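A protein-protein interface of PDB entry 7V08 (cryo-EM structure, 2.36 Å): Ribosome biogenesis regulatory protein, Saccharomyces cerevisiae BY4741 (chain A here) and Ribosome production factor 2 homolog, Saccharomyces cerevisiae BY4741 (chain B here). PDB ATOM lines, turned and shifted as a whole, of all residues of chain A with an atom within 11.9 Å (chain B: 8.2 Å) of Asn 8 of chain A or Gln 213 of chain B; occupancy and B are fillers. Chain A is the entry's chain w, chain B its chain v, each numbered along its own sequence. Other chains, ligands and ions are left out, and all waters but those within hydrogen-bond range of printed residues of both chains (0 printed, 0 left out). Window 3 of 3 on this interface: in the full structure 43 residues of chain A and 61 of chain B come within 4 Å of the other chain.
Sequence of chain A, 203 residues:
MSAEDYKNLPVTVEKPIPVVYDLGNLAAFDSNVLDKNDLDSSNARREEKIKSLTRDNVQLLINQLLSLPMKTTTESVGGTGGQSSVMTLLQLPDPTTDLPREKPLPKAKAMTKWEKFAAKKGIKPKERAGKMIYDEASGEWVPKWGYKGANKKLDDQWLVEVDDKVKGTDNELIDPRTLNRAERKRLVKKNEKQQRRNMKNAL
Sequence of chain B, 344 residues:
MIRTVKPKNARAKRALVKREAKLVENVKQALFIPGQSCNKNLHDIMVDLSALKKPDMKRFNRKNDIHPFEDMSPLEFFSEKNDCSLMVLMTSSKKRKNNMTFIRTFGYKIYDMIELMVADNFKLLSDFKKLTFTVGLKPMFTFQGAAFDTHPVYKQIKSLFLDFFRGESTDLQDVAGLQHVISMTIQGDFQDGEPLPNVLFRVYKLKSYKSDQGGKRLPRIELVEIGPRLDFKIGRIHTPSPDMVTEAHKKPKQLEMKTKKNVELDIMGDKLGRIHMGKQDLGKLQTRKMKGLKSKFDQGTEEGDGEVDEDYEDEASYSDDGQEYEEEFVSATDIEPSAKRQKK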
ATOM      1  N   ASN A   8       5.505 -18.328 -30.074  1.00  0.00           N
ATOM      2  CA  ASN A   8       4.745 -17.889 -28.909  1.00  0.00           C
ATOM      3  C   ASN A   8       3.667 -16.883 -29.307  1.00  0.00           C
ATOM      4  O   ASN A   8       3.698 -15.722 -28.907  1.00  0.00           O
ATOM      5  CB  ASN A   8       5.678 -17.298 -27.847  1.00  0.00           C
ATOM      6  CG  ASN A   8       6.696 -16.329 -28.425  1.00  0.00           C
ATOM      7  OD1 ASN A   8       6.498 -15.114 -28.404  1.00  0.00           O
ATOM      8  ND2 ASN A   8       7.805 -16.863 -28.926  1.00  0.00           N
ATOM      9  N   LEU A   9       2.711 -17.362 -30.100  1.00  0.00           N
ATOM     10  CA  LEU A   9       1.605 -16.532 -30.553  1.00  0.00           C
ATOM     11  C   LEU A   9       0.723 -16.133 -29.370  1.00  0.00           C
ATOM     12  O   LEU A   9       0.613 -16.884 -28.396  1.00  0.00           O
ATOM     13  CB  LEU A   9       0.784 -17.290 -31.596  1.00  0.00           C
ATOM     14  CG  LEU A   9       1.574 -17.797 -32.805  1.00  0.00           C
ATOM     15  CD1 LEU A   9       0.782 -18.827 -33.594  1.00  0.00           C
ATOM     16  CD2 LEU A   9       1.992 -16.639 -33.702  1.00  0.00           C
ATOM     17  N   PRO A  10       0.103 -14.955 -29.412  1.00  0.00           N
ATOM     18  CA  PRO A  10      -0.675 -14.483 -28.261  1.00  0.00           C
ATOM     19  C   PRO A  10      -1.943 -15.297 -28.050  1.00  0.00           C
ATOM     20  O   PRO A  10      -2.393 -16.044 -28.919  1.00  0.00           O
ATOM     21  CB  PRO A  10      -1.012 -13.032 -28.624  1.00  0.00           C
ATOM     22  CG  PRO A  10      -0.080 -12.675 -29.741  1.00  0.00           C
ATOM     23  CD  PRO A  10       0.174 -13.944 -30.479  1.00  0.00           C
ATOM     24  N   VAL A  11      -2.510 -15.154 -26.855  1.00  0.00           N
ATOM     25  CA  VAL A  11      -3.768 -15.795 -26.501  1.00  0.00           C
ATOM     26  C   VAL A  11      -4.871 -14.761 -26.271  1.00  0.00           C
ATOM     27  O   VAL A  11      -5.984 -15.120 -25.888  1.00  0.00           O
ATOM     28  CB  VAL A  11      -3.610 -16.712 -25.275  1.00  0.00           C
ATOM     29  CG1 VAL A  11      -2.522 -17.747 -25.510  1.00  0.00           C
ATOM     30  CG2 VAL A  11      -3.323 -15.895 -24.023  1.00  0.00           C
ATOM     31  N   THR A  12      -4.580 -13.482 -26.503  1.00  0.00           N
ATOM     32  CA  THR A  12      -5.526 -12.392 -26.283  1.00  0.00           C
ATOM     33  C   THR A  12      -6.064 -11.935 -27.635  1.00  0.00           C
ATOM     34  O   THR A  12      -5.297 -11.488 -28.493  1.00  0.00           O
ATOM     35  CB  THR A  12      -4.863 -11.238 -25.535  1.00  0.00           C
ATOM     36  OG1 THR A  12      -3.884 -10.615 -26.374  1.00  0.00           O
ATOM     37  CG2 THR A  12      -4.180 -11.755 -24.285  1.00  0.00           C
ATOM     38  N   VAL A  13      -7.378 -12.037 -27.812  1.00  0.00           N
ATOM     39  CA  VAL A  13      -8.038 -11.804 -29.093  1.00  0.00           C
ATOM     40  C   VAL A  13      -8.817 -10.495 -29.021  1.00  0.00           C
ATOM     41  O   VAL A  13      -9.592 -10.275 -28.083  1.00  0.00           O
ATOM     42  CB  VAL A  13      -8.961 -12.978 -29.461  1.00  0.00           C
ATOM     43  CG1 VAL A  13      -9.825 -12.634 -30.659  1.00  0.00           C
ATOM     44  CG2 VAL A  13      -8.140 -14.219 -29.741  1.00  0.00           C
ATOM     45  N   GLU A  14      -8.630  -9.636 -30.022  1.00  0.00           N
ATOM     46  CA  GLU A  14      -9.275  -8.331 -30.080  1.00  0.00           C
ATOM     47  C   GLU A  14     -10.503  -8.397 -30.986  1.00  0.00           C
ATOM     48  O   GLU A  14     -10.433  -8.928 -32.097  1.00  0.00           O
ATOM     49  CB  GLU A  14      -8.294  -7.270 -30.577  1.00  0.00           C
ATOM     50  CG  GLU A  14      -7.117  -7.053 -29.648  1.00  0.00           C
ATOM     51  CD  GLU A  14      -6.069  -6.123 -30.224  1.00  0.00           C
ATOM     52  OE1 GLU A  14      -6.431  -5.242 -31.030  1.00  0.00           O
ATOM     53  OE2 GLU A  14      -4.880  -6.275 -29.872  1.00  0.00           O
ATOM     54  N   ARG A  55     -11.155 -20.192 -34.706  1.00  0.00           N
ATOM     55  CA  ARG A  55     -10.032 -20.280 -33.785  1.00  0.00           C
ATOM     56  C   ARG A  55     -10.070 -19.143 -32.771  1.00  0.00           C
ATOM     57  O   ARG A  55      -9.844 -19.365 -31.578  1.00  0.00           O
ATOM     58  CB  ARG A  55      -8.727 -20.270 -34.583  1.00  0.00           C
ATOM     59  CG  ARG A  55      -7.593 -21.079 -33.995  1.00  0.00           C
ATOM     60  CD  ARG A  55      -6.954 -20.365 -32.837  1.00  0.00           C
ATOM     61  NE  ARG A  55      -6.471 -19.031 -33.166  1.00  0.00           N
ATOM     62  CZ  ARG A  55      -6.137 -18.124 -32.259  1.00  0.00           C
ATOM     63  NH1 ARG A  55      -6.211 -18.384 -30.966  1.00  0.00           N
ATOM     64  NH2 ARG A  55      -5.732 -16.923 -32.659  1.00  0.00           N
ATOM     65  N   GLN A  59     -10.702 -19.734 -28.847  1.00  0.00           N
ATOM     66  CA  GLN A  59      -9.696 -19.258 -27.902  1.00  0.00           C
ATOM     67  C   GLN A  59     -10.331 -18.451 -26.779  1.00  0.00           C
ATOM     68  O   GLN A  59     -10.019 -18.661 -25.599  1.00  0.00           O
ATOM     69  CB  GLN A  59      -8.647 -18.423 -28.633  1.00  0.00           C
ATOM     70  CG  GLN A  59      -7.609 -17.798 -27.728  1.00  0.00           C
ATOM     71  CD  GLN A  59      -6.709 -18.828 -27.085  1.00  0.00           C
ATOM     72  OE1 GLN A  59      -6.061 -19.616 -27.772  1.00  0.00           O
ATOM     73  NE2 GLN A  59      -6.668 -18.831 -25.760  1.00  0.00           N
ATOM     74  N   ASN A  63     -10.500 -19.449 -22.789  1.00  0.00           N
ATOM     75  CA  ASN A  63     -10.057 -18.546 -21.728  1.00  0.00           C
ATOM     76  C   ASN A  63     -11.115 -18.424 -20.637  1.00  0.00           C
ATOM     77  O   ASN A  63     -10.800 -18.482 -19.440  1.00  0.00           O
ATOM     78  CB  ASN A  63      -9.723 -17.170 -22.301  1.00  0.00           C
ATOM     79  CG  ASN A  63      -8.587 -17.210 -23.302  1.00  0.00           C
ATOM     80  OD1 ASN A  63      -7.867 -18.201 -23.397  1.00  0.00           O
ATOM     81  ND2 ASN A  63      -8.415 -16.124 -24.048  1.00  0.00           N
ATOM     82  N   TYR B 209      -1.058 -25.713 -27.058  1.00  0.00           N
ATOM     83  CA  TYR B 209       0.383 -25.550 -26.966  1.00  0.00           C
ATOM     84  C   TYR B 209       0.708 -24.561 -25.858  1.00  0.00           C
ATOM     85  O   TYR B 209      -0.122 -23.736 -25.470  1.00  0.00           O
ATOM     86  CB  TYR B 209       0.986 -25.057 -28.290  1.00  0.00           C
ATOM     87  CG  TYR B 209       0.707 -25.968 -29.456  1.00  0.00           C
ATOM     88  CD1 TYR B 209       1.531 -27.052 -29.727  1.00  0.00           C
ATOM     89  CD2 TYR B 209      -0.385 -25.748 -30.285  1.00  0.00           C
ATOM     90  CE1 TYR B 209       1.274 -27.889 -30.792  1.00  0.00           C
ATOM     91  CE2 TYR B 209      -0.648 -26.576 -31.346  1.00  0.00           C
ATOM     92  CZ  TYR B 209       0.185 -27.646 -31.597  1.00  0.00           C
ATOM     93  OH  TYR B 209      -0.080 -28.474 -32.662  1.00  0.00           O
ATOM     94  N   LYS B 210       1.932 -24.657 -25.349  1.00  0.00           N
ATOM     95  CA  LYS B 210       2.433 -23.657 -24.418  1.00  0.00           C
ATOM     96  C   LYS B 210       2.608 -22.327 -25.143  1.00  0.00           C
ATOM     97  O   LYS B 210       3.201 -22.266 -26.223  1.00  0.00           O
ATOM     98  CB  LYS B 210       3.758 -24.117 -23.814  1.00  0.00           C
ATOM     99  CG  LYS B 210       4.358 -23.169 -22.785  1.00  0.00           C
ATOM    100  CD  LYS B 210       3.726 -23.354 -21.414  1.00  0.00           C
ATOM    101  CE  LYS B 210       4.234 -22.313 -20.434  1.00  0.00           C
ATOM    102  NZ  LYS B 210       5.672 -22.488 -20.075  1.00  0.00           N
ATOM    103  N   SER B 211       2.085 -21.255 -24.547  1.00  0.00           N
ATOM    104  CA  SER B 211       2.077 -19.957 -25.205  1.00  0.00           C
ATOM    105  C   SER B 211       3.263 -19.077 -24.837  1.00  0.00           C
ATOM    106  O   SER B 211       3.591 -18.170 -25.606  1.00  0.00           O
ATOM    107  CB  SER B 211       0.786 -19.195 -24.880  1.00  0.00           C
ATOM    108  OG  SER B 211       0.869 -18.570 -23.611  1.00  0.00           O
ATOM    109  N   ASP B 212       3.880 -19.294 -23.674  1.00  0.00           N
ATOM    110  CA  ASP B 212       5.009 -18.525 -23.149  1.00  0.00           C
ATOM    111  C   ASP B 212       4.684 -17.046 -22.951  1.00  0.00           C
ATOM    112  O   ASP B 212       5.569 -16.263 -22.589  1.00  0.00           O
ATOM    113  CB  ASP B 212       6.256 -18.672 -24.038  1.00  0.00           C
ATOM    114  CG  ASP B 212       7.555 -18.534 -23.258  1.00  0.00           C
ATOM    115  OD1 ASP B 212       7.499 -18.440 -22.016  1.00  0.00           O
ATOM    116  OD2 ASP B 212       8.633 -18.525 -23.889  1.00  0.00           O
ATOM    117  N   GLN B 213       3.434 -16.644 -23.170  1.00  0.00           N
ATOM    118  CA  GLN B 213       2.986 -15.280 -22.933  1.00  0.00           C
ATOM    119  C   GLN B 213       1.770 -15.191 -22.034  1.00  0.00           C
ATOM    120  O   GLN B 213       1.551 -14.131 -21.436  1.00  0.00           O
ATOM    121  CB  GLN B 213       2.655 -14.579 -24.258  1.00  0.00           C
ATOM    122  CG  GLN B 213       3.859 -14.210 -25.101  1.00  0.00           C
ATOM    123  CD  GLN B 213       3.459 -13.601 -26.431  1.00  0.00           C
ATOM    124  OE1 GLN B 213       2.273 -13.451 -26.724  1.00  0.00           O
ATOM    125  NE2 GLN B 213       4.448 -13.245 -27.242  1.00  0.00           N
ATOM    126  N   GLY B 214       0.961 -16.242 -21.941  1.00  0.00           N
ATOM    127  CA  GLY B 214      -0.164 -16.273 -21.031  1.00  0.00           C
ATOM    128  C   GLY B 214       0.096 -17.153 -19.827  1.00  0.00           C
ATOM    129  O   GLY B 214      -0.837 -17.532 -19.113  1.00  0.00           O
ATOM    130  N   GLY B 215       1.362 -17.491 -19.599  1.00  0.00           N
ATOM    131  CA  GLY B 215       1.727 -18.341 -18.488  1.00  0.00           C
ATOM    132  C   GLY B 215       1.399 -19.798 -18.756  1.00  0.00           C
ATOM    133  O   GLY B 215       1.023 -20.198 -19.862  1.00  0.00           O
ATOM    134  N   LYS B 216       1.538 -20.602 -17.708  1.00  0.00           N
ATOM    135  CA  LYS B 216       1.234 -22.021 -17.784  1.00  0.00           C
ATOM    136  C   LYS B 216      -0.250 -22.310 -17.614  1.00  0.00           C
ATOM    137  O   LYS B 216      -0.676 -23.448 -17.826  1.00  0.00           O
ATOM    138  CB  LYS B 216       2.046 -22.792 -16.739  1.00  0.00           C
ATOM    139  CG  LYS B 216       1.816 -22.350 -15.305  1.00  0.00           C
ATOM    140  CD  LYS B 216       2.667 -23.149 -14.320  1.00  0.00           C
ATOM    141  CE  LYS B 216       2.417 -24.646 -14.444  1.00  0.00           C
ATOM    142  NZ  LYS B 216       0.969 -24.982 -14.343  1.00  0.00           N
ATOM    143  N   LEU B 218      -2.768 -20.456 -19.261  1.00  0.00           N
ATOM    144  CA  LEU B 218      -3.494 -20.091 -20.478  1.00  0.00           C
ATOM    145  C   LEU B 218      -2.700 -20.543 -21.696  1.00  0.00           C
ATOM    146  O   LEU B 218      -1.639 -19.969 -21.996  1.00  0.00           O
ATOM    147  CB  LEU B 218      -3.755 -18.593 -20.532  1.00  0.00           C
ATOM    148  CG  LEU B 218      -4.527 -18.019 -19.350  1.00  0.00           C
ATOM    149  CD1 LEU B 218      -4.453 -16.505 -19.360  1.00  0.00           C
ATOM    150  CD2 LEU B 218      -5.965 -18.485 -19.404  1.00  0.00           C
ATOM    151  N   PRO B 219      -3.164 -21.565 -22.409  1.00  0.00           N
ATOM    152  CA  PRO B 219      -2.442 -22.055 -23.583  1.00  0.00           C
ATOM    153  C   PRO B 219      -2.926 -21.409 -24.874  1.00  0.00           C
ATOM    154  O   PRO B 219      -3.983 -20.779 -24.935  1.00  0.00           O
ATOM    155  CB  PRO B 219      -2.777 -23.552 -23.573  1.00  0.00           C
ATOM    156  CG  PRO B 219      -4.178 -23.574 -23.070  1.00  0.00           C
ATOM    157  CD  PRO B 219      -4.320 -22.420 -22.095  1.00  0.00           C
ATOM    158  N   ARG B 220      -2.123 -21.587 -25.920  1.00  0.00           N
ATOM    159  CA  ARG B 220      -2.538 -21.198 -27.262  1.00  0.00           C
ATOM    160  C   ARG B 220      -3.329 -22.325 -27.910  1.00  0.00           C
ATOM    161  O   ARG B 220      -2.872 -23.471 -27.958  1.00  0.00           O
ATOM    162  CB  ARG B 220      -1.323 -20.851 -28.120  1.00  0.00           C
ATOM    163  CG  ARG B 220      -1.636 -20.599 -29.595  1.00  0.00           C
ATOM    164  CD  ARG B 220      -2.196 -19.204 -29.833  1.00  0.00           C
ATOM    165  NE  ARG B 220      -2.285 -18.896 -31.256  1.00  0.00           N
ATOM    166  CZ  ARG B 220      -2.732 -17.751 -31.755  1.00  0.00           C
ATOM    167  NH1 ARG B 220      -3.160 -16.773 -30.973  1.00  0.00           N
ATOM    168  NH2 ARG B 220      -2.746 -17.582 -33.074  1.00  0.00           N
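Hydrophobic or aromatic side chains of chain A that line the printed part of chain B: Leu 9, Pro 10 and Val 11. Among the printed residues, 11 pairs touch across the chains.
CB of Asn 8 of chain A touches O of Ser 211 of chain B, at 3.2 Å. Leu 9 of chain A touches Arg 220 of chain B. Pro 10 of chain A touches Gln 213 of chain B. Val 11 of chain A touches Ser 211 of chain B (CG1 to CB, 3.7 Å). O of Pro 219 of chain B touches CG1 of Val 11 of chain A, at 3.4 Å. CG1 of Val 11 of chain A touches CA of Arg 220 of chain B, 3.9 Å away. Gln 59 of chain A touches Arg 220 of chain B (OE1 to C, 3.8 Å).
Asn 8 of chain A touches two residues of chain B. Of chain A, only Asn 8 (3.2 Å) and Val 11 (3.7 Å) come within 4 Å of Ser 211 of chain B. No residue of chain A comes within 4 Å of Asp 212 of chain B. No residue of chain A comes within 4 Å of Gly 214 of chain B. Of the printed residues of chain B, Val 11 of chain A touches Ser 211 (3.7 Å), Pro 219 (3.4 Å) and Arg 220 (3.9 Å). Printed residues of chain A within 4 Å of Pro 219 of chain B: Val 11 (3.4 Å) and Gln 59 (3.4 Å). Printed residues of chain B within 4 Å of Pro 10 of chain A: Gln 213 (3.5 Å) and Arg 220 (2.3 Å). Of the printed residues of chain B, Arg 55 of chain A touches Arg 220. Printed residues of chain A within 4 Å of Arg 220 of chain B: Leu 9, Pro 10, Val 11, Arg 55 and Gln 59. The nearest residue of chain B that does not touch Asn 8 of chain A is Asp 212 of chain B (4.1 Å). The nearest printed residue of chain A that does not touch Pro 219 of chain B is Asn 63 of chain A (4.9 Å).
The backbone carbonyl oxygen (O) of Tyr 209 of chain B is in hydrogen-bond range of the backbone NH (N) of Arg 220 of chain B, at 3.0 Å. The side-chain hydroxyl of Ser 211 of chain B sits close to the backbone NH of Gln 213 of chain B, at 3.2 Å. OG of Ser 211 of chain B sits at hydrogen-bond distance from N of Gly 214 of chain B, at 2.9 Å. The side-chain hydroxyl of Ser 211 of chain B is in hydrogen-bond range of the backbone carbonyl oxygen of Leu 218 of chain B (3.3 Å). O of Val 11 of chain A sits at hydrogen-bond distance from ND2 of Asn 63 of chain A, at 3.2 Å. OE1 of Gln 59 of chain A sits close to NH1 of Arg 55 of chain A (3.4 Å).
NE2 of Gln 213 of chain B is in hydrogen-bond range of OD1 of Asn 8 of chain A (3.0 Å). The backbone carbonyl oxygen (O) of Pro 219 of chain B is in hydrogen-bond range of the side-chain amide nitrogen (NE2) of Gln 59 of chain A (3.4 Å). The guanidinium group (NH1) of Arg 220 of chain B sits close to the backbone carbonyl oxygen (O) of Pro 10 of chain A. The guanidinium group (NH2) of Arg 55 of chain A sits close to the guanidinium group (NH1) of Arg 220 of chain B (3.1 Å).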
